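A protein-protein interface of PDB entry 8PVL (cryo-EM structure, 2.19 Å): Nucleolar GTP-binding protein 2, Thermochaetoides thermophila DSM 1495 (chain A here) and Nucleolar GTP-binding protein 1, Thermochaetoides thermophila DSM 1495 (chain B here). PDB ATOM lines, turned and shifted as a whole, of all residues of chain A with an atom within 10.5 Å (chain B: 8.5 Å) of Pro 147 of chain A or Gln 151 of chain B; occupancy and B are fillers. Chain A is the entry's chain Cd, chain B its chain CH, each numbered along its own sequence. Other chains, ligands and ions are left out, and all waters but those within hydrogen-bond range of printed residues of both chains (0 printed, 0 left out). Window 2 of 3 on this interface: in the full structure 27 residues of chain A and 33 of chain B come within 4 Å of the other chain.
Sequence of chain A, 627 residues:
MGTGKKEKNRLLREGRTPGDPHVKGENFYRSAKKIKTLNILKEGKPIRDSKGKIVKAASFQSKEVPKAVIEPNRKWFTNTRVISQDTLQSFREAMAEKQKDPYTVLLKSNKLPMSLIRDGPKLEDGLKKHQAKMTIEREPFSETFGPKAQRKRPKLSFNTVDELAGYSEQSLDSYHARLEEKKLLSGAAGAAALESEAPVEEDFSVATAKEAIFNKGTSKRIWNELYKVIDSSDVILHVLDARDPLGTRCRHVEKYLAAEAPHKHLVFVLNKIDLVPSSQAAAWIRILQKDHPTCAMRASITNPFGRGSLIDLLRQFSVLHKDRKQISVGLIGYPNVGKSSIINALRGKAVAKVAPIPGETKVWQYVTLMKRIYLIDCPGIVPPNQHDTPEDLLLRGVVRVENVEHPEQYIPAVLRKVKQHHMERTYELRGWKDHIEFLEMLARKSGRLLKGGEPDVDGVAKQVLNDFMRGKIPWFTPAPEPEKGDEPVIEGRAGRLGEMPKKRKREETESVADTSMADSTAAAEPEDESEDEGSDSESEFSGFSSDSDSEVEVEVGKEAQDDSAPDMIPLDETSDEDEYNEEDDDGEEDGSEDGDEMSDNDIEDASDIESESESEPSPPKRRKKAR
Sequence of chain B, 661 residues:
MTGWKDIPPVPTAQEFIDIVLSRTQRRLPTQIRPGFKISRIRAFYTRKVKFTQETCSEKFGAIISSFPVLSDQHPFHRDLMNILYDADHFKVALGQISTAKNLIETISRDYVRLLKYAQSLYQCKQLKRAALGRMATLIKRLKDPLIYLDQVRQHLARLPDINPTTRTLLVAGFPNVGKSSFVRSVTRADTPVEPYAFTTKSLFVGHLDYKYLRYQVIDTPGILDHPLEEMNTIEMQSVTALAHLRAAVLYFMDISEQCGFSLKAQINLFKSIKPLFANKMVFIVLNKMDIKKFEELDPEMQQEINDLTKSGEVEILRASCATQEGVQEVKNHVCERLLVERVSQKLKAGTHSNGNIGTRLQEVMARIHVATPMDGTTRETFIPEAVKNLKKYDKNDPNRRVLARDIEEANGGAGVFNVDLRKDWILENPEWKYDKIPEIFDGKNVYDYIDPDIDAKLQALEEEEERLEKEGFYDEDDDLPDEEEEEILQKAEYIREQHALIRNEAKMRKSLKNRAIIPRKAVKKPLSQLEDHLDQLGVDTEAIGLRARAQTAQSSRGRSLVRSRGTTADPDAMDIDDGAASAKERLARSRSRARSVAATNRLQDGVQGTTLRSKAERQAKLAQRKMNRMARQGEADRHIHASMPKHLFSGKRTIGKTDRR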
ATOM      1  N   PHE A 141      13.383  -0.239   9.110  1.00  0.00           N
ATOM      2  CA  PHE A 141      14.065   0.996   8.730  1.00  0.00           C
ATOM      3  C   PHE A 141      14.932   1.544   9.856  1.00  0.00           C
ATOM      4  O   PHE A 141      15.984   2.136   9.590  1.00  0.00           O
ATOM      5  CB  PHE A 141      13.046   2.050   8.301  1.00  0.00           C
ATOM      6  CG  PHE A 141      12.483   1.832   6.928  1.00  0.00           C
ATOM      7  CD1 PHE A 141      13.309   1.844   5.815  1.00  0.00           C
ATOM      8  CD2 PHE A 141      11.126   1.624   6.749  1.00  0.00           C
ATOM      9  CE1 PHE A 141      12.790   1.648   4.551  1.00  0.00           C
ATOM     10  CE2 PHE A 141      10.603   1.428   5.488  1.00  0.00           C
ATOM     11  CZ  PHE A 141      11.436   1.444   4.387  1.00  0.00           C
ATOM     12  N   SER A 142      14.512   1.367  11.110  1.00  0.00           N
ATOM     13  CA  SER A 142      15.294   1.875  12.232  1.00  0.00           C
ATOM     14  C   SER A 142      16.560   1.066  12.475  1.00  0.00           C
ATOM     15  O   SER A 142      17.511   1.592  13.062  1.00  0.00           O
ATOM     16  CB  SER A 142      14.438   1.902  13.498  1.00  0.00           C
ATOM     17  OG  SER A 142      14.010   0.600  13.851  1.00  0.00           O
ATOM     18  N   GLU A 143      16.596  -0.195  12.047  1.00  0.00           N
ATOM     19  CA  GLU A 143      17.797  -1.007  12.176  1.00  0.00           C
ATOM     20  C   GLU A 143      18.738  -0.874  10.988  1.00  0.00           C
ATOM     21  O   GLU A 143      19.876  -1.346  11.064  1.00  0.00           O
ATOM     22  CB  GLU A 143      17.423  -2.482  12.357  1.00  0.00           C
ATOM     23  CG  GLU A 143      16.767  -2.805  13.687  1.00  0.00           C
ATOM     24  CD  GLU A 143      16.409  -4.272  13.817  1.00  0.00           C
ATOM     25  OE1 GLU A 143      16.716  -5.046  12.886  1.00  0.00           O
ATOM     26  OE2 GLU A 143      15.817  -4.652  14.848  1.00  0.00           O
ATOM     27  N   THR A 144      18.294  -0.245   9.899  1.00  0.00           N
ATOM     28  CA  THR A 144      19.129  -0.125   8.710  1.00  0.00           C
ATOM     29  C   THR A 144      19.976   1.142   8.750  1.00  0.00           C
ATOM     30  O   THR A 144      21.202   1.083   8.613  1.00  0.00           O
ATOM     31  CB  THR A 144      18.254  -0.148   7.454  1.00  0.00           C
ATOM     32  OG1 THR A 144      17.639  -1.435   7.322  1.00  0.00           O
ATOM     33  CG2 THR A 144      19.084   0.138   6.214  1.00  0.00           C
ATOM     34  N   PHE A 145      19.338   2.294   8.935  1.00  0.00           N
ATOM     35  CA  PHE A 145      20.041   3.566   8.996  1.00  0.00           C
ATOM     36  C   PHE A 145      19.401   4.416  10.081  1.00  0.00           C
ATOM     37  O   PHE A 145      18.182   4.384  10.263  1.00  0.00           O
ATOM     38  CB  PHE A 145      20.000   4.293   7.647  1.00  0.00           C
ATOM     39  CG  PHE A 145      21.004   5.400   7.523  1.00  0.00           C
ATOM     40  CD1 PHE A 145      22.334   5.119   7.259  1.00  0.00           C
ATOM     41  CD2 PHE A 145      20.620   6.724   7.666  1.00  0.00           C
ATOM     42  CE1 PHE A 145      23.262   6.131   7.145  1.00  0.00           C
ATOM     43  CE2 PHE A 145      21.544   7.743   7.553  1.00  0.00           C
ATOM     44  CZ  PHE A 145      22.866   7.445   7.292  1.00  0.00           C
ATOM     45  N   GLY A 146      20.226   5.168  10.802  1.00  0.00           N
ATOM     46  CA  GLY A 146      19.741   6.027  11.854  1.00  0.00           C
ATOM     47  C   GLY A 146      20.584   5.951  13.110  1.00  0.00           C
ATOM     48  O   GLY A 146      21.597   5.249  13.164  1.00  0.00           O
ATOM     49  N   PRO A 147      20.181   6.696  14.146  1.00  0.00           N
ATOM     50  CA  PRO A 147      20.953   6.696  15.401  1.00  0.00           C
ATOM     51  C   PRO A 147      20.965   5.363  16.129  1.00  0.00           C
ATOM     52  O   PRO A 147      21.889   5.120  16.915  1.00  0.00           O
ATOM     53  CB  PRO A 147      20.259   7.778  16.240  1.00  0.00           C
ATOM     54  CG  PRO A 147      18.895   7.905  15.650  1.00  0.00           C
ATOM     55  CD  PRO A 147      19.057   7.645  14.188  1.00  0.00           C
ATOM     56  N   LYS A 148      19.980   4.493  15.902  1.00  0.00           N
ATOM     57  CA  LYS A 148      19.918   3.191  16.552  1.00  0.00           C
ATOM     58  C   LYS A 148      20.152   2.044  15.575  1.00  0.00           C
ATOM     59  O   LYS A 148      19.759   0.909  15.855  1.00  0.00           O
ATOM     60  CB  LYS A 148      18.573   3.009  17.256  1.00  0.00           C
ATOM     61  CG  LYS A 148      18.174   4.146  18.182  1.00  0.00           C
ATOM     62  CD  LYS A 148      19.250   4.438  19.214  1.00  0.00           C
ATOM     63  CE  LYS A 148      18.944   5.715  19.979  1.00  0.00           C
ATOM     64  NZ  LYS A 148      20.071   6.112  20.866  1.00  0.00           N
ATOM     65  N   ALA A 149      20.781   2.320  14.435  1.00  0.00           N
ATOM     66  CA  ALA A 149      20.957   1.306  13.406  1.00  0.00           C
ATOM     67  C   ALA A 149      21.978   0.259  13.832  1.00  0.00           C
ATOM     68  O   ALA A 149      23.006   0.576  14.435  1.00  0.00           O
ATOM     69  CB  ALA A 149      21.394   1.950  12.093  1.00  0.00           C
ATOM     70  N   GLN A 150      21.688  -1.000  13.504  1.00  0.00           N
ATOM     71  CA  GLN A 150      22.564  -2.120  13.823  1.00  0.00           C
ATOM     72  C   GLN A 150      23.130  -2.787  12.577  1.00  0.00           C
ATOM     73  O   GLN A 150      23.798  -3.821  12.692  1.00  0.00           O
ATOM     74  CB  GLN A 150      21.819  -3.152  14.673  1.00  0.00           C
ATOM     75  CG  GLN A 150      21.258  -2.599  15.969  1.00  0.00           C
ATOM     76  CD  GLN A 150      22.333  -2.046  16.880  1.00  0.00           C
ATOM     77  OE1 GLN A 150      23.277  -2.746  17.240  1.00  0.00           O
ATOM     78  NE2 GLN A 150      22.194  -0.783  17.259  1.00  0.00           N
ATOM     79  N   ARG A 151      22.873  -2.232  11.395  1.00  0.00           N
ATOM     80  CA  ARG A 151      23.354  -2.824  10.154  1.00  0.00           C
ATOM     81  C   ARG A 151      24.860  -2.640  10.028  1.00  0.00           C
ATOM     82  O   ARG A 151      25.377  -1.531  10.180  1.00  0.00           O
ATOM     83  CB  ARG A 151      22.632  -2.193   8.965  1.00  0.00           C
ATOM     84  CG  ARG A 151      23.243  -2.477   7.604  1.00  0.00           C
ATOM     85  CD  ARG A 151      22.462  -1.754   6.521  1.00  0.00           C
ATOM     86  NE  ARG A 151      23.036  -1.922   5.191  1.00  0.00           N
ATOM     87  CZ  ARG A 151      23.818  -1.034   4.594  1.00  0.00           C
ATOM     88  NH1 ARG A 151      24.173   0.089   5.193  1.00  0.00           N
ATOM     89  NH2 ARG A 151      24.254  -1.278   3.361  1.00  0.00           N
ATOM     90  N   VAL B  10      12.414  16.322   5.593  1.00  0.00           N
ATOM     91  CA  VAL B  10      11.365  15.309   5.569  1.00  0.00           C
ATOM     92  C   VAL B  10      10.729  15.270   6.955  1.00  0.00           C
ATOM     93  O   VAL B  10      11.389  14.839   7.914  1.00  0.00           O
ATOM     94  CB  VAL B  10      11.919  13.935   5.173  1.00  0.00           C
ATOM     95  CG1 VAL B  10      10.805  12.910   5.123  1.00  0.00           C
ATOM     96  CG2 VAL B  10      12.634  14.018   3.835  1.00  0.00           C
ATOM     97  N   PHE B  67      15.180  13.589  -4.115  1.00  0.00           N
ATOM     98  CA  PHE B  67      16.095  12.513  -3.779  1.00  0.00           C
ATOM     99  C   PHE B  67      16.779  11.980  -5.038  1.00  0.00           C
ATOM    100  O   PHE B  67      16.209  12.035  -6.131  1.00  0.00           O
ATOM    101  CB  PHE B  67      15.354  11.386  -3.063  1.00  0.00           C
ATOM    102  CG  PHE B  67      15.385  11.503  -1.566  1.00  0.00           C
ATOM    103  CD1 PHE B  67      14.488  12.323  -0.904  1.00  0.00           C
ATOM    104  CD2 PHE B  67      16.319  10.803  -0.823  1.00  0.00           C
ATOM    105  CE1 PHE B  67      14.517  12.437   0.472  1.00  0.00           C
ATOM    106  CE2 PHE B  67      16.355  10.914   0.553  1.00  0.00           C
ATOM    107  CZ  PHE B  67      15.452  11.732   1.201  1.00  0.00           C
ATOM    108  N   TYR B  85      23.441   3.361   2.691  1.00  0.00           N
ATOM    109  CA  TYR B  85      22.071   3.000   3.021  1.00  0.00           C
ATOM    110  C   TYR B  85      21.672   1.849   2.118  1.00  0.00           C
ATOM    111  O   TYR B  85      22.023   1.847   0.939  1.00  0.00           O
ATOM    112  CB  TYR B  85      21.121   4.186   2.822  1.00  0.00           C
ATOM    113  CG  TYR B  85      21.835   5.509   2.656  1.00  0.00           C
ATOM    114  CD1 TYR B  85      22.274   6.227   3.760  1.00  0.00           C
ATOM    115  CD2 TYR B  85      22.085   6.031   1.395  1.00  0.00           C
ATOM    116  CE1 TYR B  85      22.936   7.429   3.614  1.00  0.00           C
ATOM    117  CE2 TYR B  85      22.746   7.232   1.238  1.00  0.00           C
ATOM    118  CZ  TYR B  85      23.168   7.928   2.351  1.00  0.00           C
ATOM    119  OH  TYR B  85      23.825   9.125   2.202  1.00  0.00           O
ATOM    120  N   ASP B 144       7.712   5.098   9.593  1.00  0.00           N
ATOM    121  CA  ASP B 144       9.106   4.658   9.533  1.00  0.00           C
ATOM    122  C   ASP B 144       9.859   5.080   8.262  1.00  0.00           C
ATOM    123  O   ASP B 144      11.033   5.477   8.376  1.00  0.00           O
ATOM    124  CB  ASP B 144       9.176   3.138   9.724  1.00  0.00           C
ATOM    125  CG  ASP B 144       8.557   2.687  11.032  1.00  0.00           C
ATOM    126  OD1 ASP B 144       8.598   3.463  12.009  1.00  0.00           O
ATOM    127  OD2 ASP B 144       8.022   1.561  11.083  1.00  0.00           O
ATOM    128  N   PRO B 145       9.273   5.004   7.046  1.00  0.00           N
ATOM    129  CA  PRO B 145       9.994   5.545   5.877  1.00  0.00           C
ATOM    130  C   PRO B 145      10.328   7.022   5.971  1.00  0.00           C
ATOM    131  O   PRO B 145      11.382   7.426   5.472  1.00  0.00           O
ATOM    132  CB  PRO B 145       9.033   5.272   4.712  1.00  0.00           C
ATOM    133  CG  PRO B 145       8.265   4.130   5.129  1.00  0.00           C
ATOM    134  CD  PRO B 145       8.067   4.271   6.595  1.00  0.00           C
ATOM    135  N   LEU B 146       9.480   7.838   6.602  1.00  0.00           N
ATOM    136  CA  LEU B 146       9.774   9.265   6.705  1.00  0.00           C
ATOM    137  C   LEU B 146      10.966   9.530   7.620  1.00  0.00           C
ATOM    138  O   LEU B 146      11.817  10.373   7.308  1.00  0.00           O
ATOM    139  CB  LEU B 146       8.537  10.017   7.191  1.00  0.00           C
ATOM    140  CG  LEU B 146       7.371  10.080   6.198  1.00  0.00           C
ATOM    141  CD1 LEU B 146       6.134  10.671   6.848  1.00  0.00           C
ATOM    142  CD2 LEU B 146       7.740  10.845   4.943  1.00  0.00           C
ATOM    143  N   ILE B 147      11.048   8.811   8.744  1.00  0.00           N
ATOM    144  CA  ILE B 147      12.190   8.935   9.651  1.00  0.00           C
ATOM    145  C   ILE B 147      13.472   8.498   8.950  1.00  0.00           C
ATOM    146  O   ILE B 147      14.510   9.181   9.010  1.00  0.00           O
ATOM    147  CB  ILE B 147      11.936   8.114  10.929  1.00  0.00           C
ATOM    148  CG1 ILE B 147      10.853   8.768  11.787  1.00  0.00           C
ATOM    149  CG2 ILE B 147      13.213   7.937  11.735  1.00  0.00           C
ATOM    150  CD1 ILE B 147      10.201   7.815  12.760  1.00  0.00           C
ATOM    151  N   TYR B 148      13.400   7.359   8.248  1.00  0.00           N
ATOM    152  CA  TYR B 148      14.550   6.854   7.507  1.00  0.00           C
ATOM    153  C   TYR B 148      15.001   7.842   6.435  1.00  0.00           C
ATOM    154  O   TYR B 148      16.203   8.100   6.281  1.00  0.00           O
ATOM    155  CB  TYR B 148      14.199   5.498   6.891  1.00  0.00           C
ATOM    156  CG  TYR B 148      15.184   4.978   5.873  1.00  0.00           C
ATOM    157  CD1 TYR B 148      16.347   4.338   6.271  1.00  0.00           C
ATOM    158  CD2 TYR B 148      14.937   5.102   4.510  1.00  0.00           C
ATOM    159  CE1 TYR B 148      17.245   3.854   5.346  1.00  0.00           C
ATOM    160  CE2 TYR B 148      15.830   4.623   3.578  1.00  0.00           C
ATOM    161  CZ  TYR B 148      16.982   3.997   4.002  1.00  0.00           C
ATOM    162  OH  TYR B 148      17.878   3.513   3.081  1.00  0.00           O
ATOM    163  N   LEU B 149      14.047   8.432   5.711  1.00  0.00           N
ATOM    164  CA  LEU B 149      14.384   9.361   4.642  1.00  0.00           C
ATOM    165  C   LEU B 149      14.945  10.669   5.179  1.00  0.00           C
ATOM    166  O   LEU B 149      15.801  11.272   4.532  1.00  0.00           O
ATOM    167  CB  LEU B 149      13.161   9.626   3.767  1.00  0.00           C
ATOM    168  CG  LEU B 149      12.822   8.546   2.737  1.00  0.00           C
ATOM    169  CD1 LEU B 149      11.472   8.815   2.097  1.00  0.00           C
ATOM    170  CD2 LEU B 149      13.908   8.438   1.685  1.00  0.00           C
ATOM    171  N   ASP B 150      14.488  11.121   6.351  1.00  0.00           N
ATOM    172  CA  ASP B 150      15.073  12.324   6.940  1.00  0.00           C
ATOM    173  C   ASP B 150      16.526  12.094   7.347  1.00  0.00           C
ATOM    174  O   ASP B 150      17.392  12.951   7.100  1.00  0.00           O
ATOM    175  CB  ASP B 150      14.243  12.782   8.137  1.00  0.00           C
ATOM    176  CG  ASP B 150      14.522  14.220   8.519  1.00  0.00           C
ATOM    177  OD1 ASP B 150      14.652  15.065   7.610  1.00  0.00           O
ATOM    178  OD2 ASP B 150      14.618  14.506   9.730  1.00  0.00           O
ATOM    179  N   GLN B 151      16.815  10.936   7.958  1.00  0.00           N
ATOM    180  CA  GLN B 151      18.201  10.610   8.295  1.00  0.00           C
ATOM    181  C   GLN B 151      19.076  10.518   7.046  1.00  0.00           C
ATOM    182  O   GLN B 151      20.195  11.059   7.010  1.00  0.00           O
ATOM    183  CB  GLN B 151      18.255   9.299   9.080  1.00  0.00           C
ATOM    184  CG  GLN B 151      17.625   9.366  10.458  1.00  0.00           C
ATOM    185  CD  GLN B 151      18.398  10.255  11.409  1.00  0.00           C
ATOM    186  OE1 GLN B 151      19.626  10.312  11.364  1.00  0.00           O
ATOM    187  NE2 GLN B 151      17.681  10.957  12.277  1.00  0.00           N
ATOM    188  N   VAL B 152      18.563   9.863   6.000  1.00  0.00           N
ATOM    189  CA  VAL B 152      19.312   9.721   4.755  1.00  0.00           C
ATOM    190  C   VAL B 152      19.523  11.080   4.093  1.00  0.00           C
ATOM    191  O   VAL B 152      20.590  11.345   3.526  1.00  0.00           O
ATOM    192  CB  VAL B 152      18.595   8.718   3.827  1.00  0.00           C
ATOM    193  CG1 VAL B 152      19.145   8.764   2.410  1.00  0.00           C
ATOM    194  CG2 VAL B 152      18.730   7.312   4.379  1.00  0.00           C
ATOM    195  N   ARG B 153      18.529  11.970   4.181  1.00  0.00           N
ATOM    196  CA  ARG B 153      18.662  13.311   3.619  1.00  0.00           C
ATOM    197  C   ARG B 153      19.763  14.102   4.311  1.00  0.00           C
ATOM    198  O   ARG B 153      20.554  14.781   3.646  1.00  0.00           O
ATOM    199  CB  ARG B 153      17.335  14.064   3.728  1.00  0.00           C
ATOM    200  CG  ARG B 153      17.468  15.562   3.495  1.00  0.00           C
ATOM    201  CD  ARG B 153      16.335  16.350   4.100  1.00  0.00           C
ATOM    202  NE  ARG B 153      16.475  16.561   5.535  1.00  0.00           N
ATOM    203  CZ  ARG B 153      17.090  17.599   6.084  1.00  0.00           C
ATOM    204  NH1 ARG B 153      17.699  18.511   5.346  1.00  0.00           N
ATOM    205  NH2 ARG B 153      17.094  17.726   7.407  1.00  0.00           N
ATOM    206  N   GLN B 154      19.829  14.029   5.644  1.00  0.00           N
ATOM    207  CA  GLN B 154      20.888  14.748   6.351  1.00  0.00           C
ATOM    208  C   GLN B 154      22.270  14.203   5.996  1.00  0.00           C
ATOM    209  O   GLN B 154      23.214  14.979   5.760  1.00  0.00           O
ATOM    210  CB  GLN B 154      20.648  14.690   7.859  1.00  0.00           C
ATOM    211  CG  GLN B 154      19.412  15.452   8.298  1.00  0.00           C
ATOM    212  CD  GLN B 154      19.328  15.633   9.798  1.00  0.00           C
ATOM    213  OE1 GLN B 154      20.303  15.427  10.517  1.00  0.00           O
ATOM    214  NE2 GLN B 154      18.155  16.026  10.278  1.00  0.00           N
ATOM    215  N   HIS B 155      22.399  12.873   5.907  1.00  0.00           N
ATOM    216  CA  HIS B 155      23.689  12.300   5.523  1.00  0.00           C
ATOM    217  C   HIS B 155      24.072  12.671   4.090  1.00  0.00           C
ATOM    218  O   HIS B 155      25.242  12.967   3.811  1.00  0.00           O
ATOM    219  CB  HIS B 155      23.669  10.784   5.698  1.00  0.00           C
ATOM    220  CG  HIS B 155      25.033  10.171   5.725  1.00  0.00           C
ATOM    221  ND1 HIS B 155      25.660   9.702   4.592  1.00  0.00           N
ATOM    222  CD2 HIS B 155      25.898   9.967   6.745  1.00  0.00           C
ATOM    223  CE1 HIS B 155      26.850   9.227   4.915  1.00  0.00           C
ATOM    224  NE2 HIS B 155      27.018   9.376   6.216  1.00  0.00           N
ATOM    225  N   LEU B 156      23.100  12.668   3.173  1.00  0.00           N
ATOM    226  CA  LEU B 156      23.367  13.048   1.789  1.00  0.00           C
ATOM    227  C   LEU B 156      23.762  14.514   1.685  1.00  0.00           C
ATOM    228  O   LEU B 156      24.620  14.876   0.873  1.00  0.00           O
ATOM    229  CB  LEU B 156      22.138  12.774   0.924  1.00  0.00           C
ATOM    230  CG  LEU B 156      21.928  11.365   0.375  1.00  0.00           C
ATOM    231  CD1 LEU B 156      20.508  11.215  -0.138  1.00  0.00           C
ATOM    232  CD2 LEU B 156      22.925  11.063  -0.725  1.00  0.00           C
ATOM    233  N   ALA B 157      23.136  15.371   2.496  1.00  0.00           N
ATOM    234  CA  ALA B 157      23.498  16.783   2.515  1.00  0.00           C
ATOM    235  C   ALA B 157      24.913  16.988   3.028  1.00  0.00           C
ATOM    236  O   ALA B 157      25.592  17.929   2.606  1.00  0.00           O
ATOM    237  CB  ALA B 157      22.508  17.571   3.370  1.00  0.00           C
ATOM    238  N   ARG B 158      25.374  16.131   3.936  1.00  0.00           N
ATOM    239  CA  ARG B 158      26.745  16.240   4.420  1.00  0.00           C
ATOM    240  C   ARG B 158      27.740  15.381   3.645  1.00  0.00           C
ATOM    241  O   ARG B 158      28.917  15.348   4.013  1.00  0.00           O
ATOM    242  CB  ARG B 158      26.805  15.898   5.907  1.00  0.00           C
ATOM    243  CG  ARG B 158      25.891  16.756   6.753  1.00  0.00           C
ATOM    244  CD  ARG B 158      26.242  16.656   8.215  1.00  0.00           C
ATOM    245  NE  ARG B 158      26.350  15.270   8.652  1.00  0.00           N
ATOM    246  CZ  ARG B 158      25.333  14.544   9.091  1.00  0.00           C
ATOM    247  NH1 ARG B 158      24.112  15.044   9.172  1.00  0.00           N
ATOM    248  NH2 ARG B 158      25.547  13.285   9.456  1.00  0.00           N
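OH of Tyr 85 of chain B lies within hydrogen-bond range of ND1 of His 155 of chain B (3.1 Å).
Asp 144 of chain B touches Phe 141 of chain A. CE2 of Phe 141 of chain A touches CG of Pro 145 of chain B, 3.6 Å away. CD1 of Phe 141 of chain A touches CG of Tyr 148 of chain B (3.7 Å). Phe 145 of chain A touches Tyr 85 of chain B (CE1 to CD1, 3.5 Å). Phe 145 of chain A touches Tyr 148 of chain B. O of Gln 151 of chain B touches CE2 of Phe 145 of chain A, at 3.6 Å. Phe 145 of chain A touches Val 152 of chain B. Phe 145 of chain A touches His 155 of chain B (CZ to CB, 3.8 Å). CD of Gln 151 of chain B touches CD of Pro 147 of chain A (3.9 Å).
Along chain A the printed residues that touch a printed residue of chain B span positions 141 to 147. Printed residues of chain B that touch a printed residue of chain A: Tyr 85, Asp 144, Pro 145, Tyr 148, Gln 151, Val 152 and His 155. Hydrophobic or aromatic side chains of chain B that line the printed part of chain A: Tyr 85, Pro 145, Tyr 148, Val 152 and His 155. Among the printed residues, 9 pairs touch across the chains.
Thr 144 of chain A touches none of the printed residues of chain B. Of the printed residues of chain B, Phe 145 of chain A touches Tyr 85, Tyr 148, Gln 151, Val 152 and His 155. Gly 146 of chain A touches none of the printed residues of chain B. Of chain B, only Gln 151 (3.9 Å) comes within 4 Å of Pro 147 of chain A. Of the printed residues of chain A, Pro 145 of chain B touches Phe 141 (3.6 Å). No residue of chain A comes within 4 Å of Asp 150 of chain B. Gln 151 of chain B touches two residues of chain A. Of chain A, only Phe 145 comes within 4 Å of Val 152 of chain B. No residue of chain A comes within 4 Å of Gln 154 of chain B. The nearest residue of chain B that does not touch Pro 147 of chain A is Ile 147 of chain B (6.3 Å).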
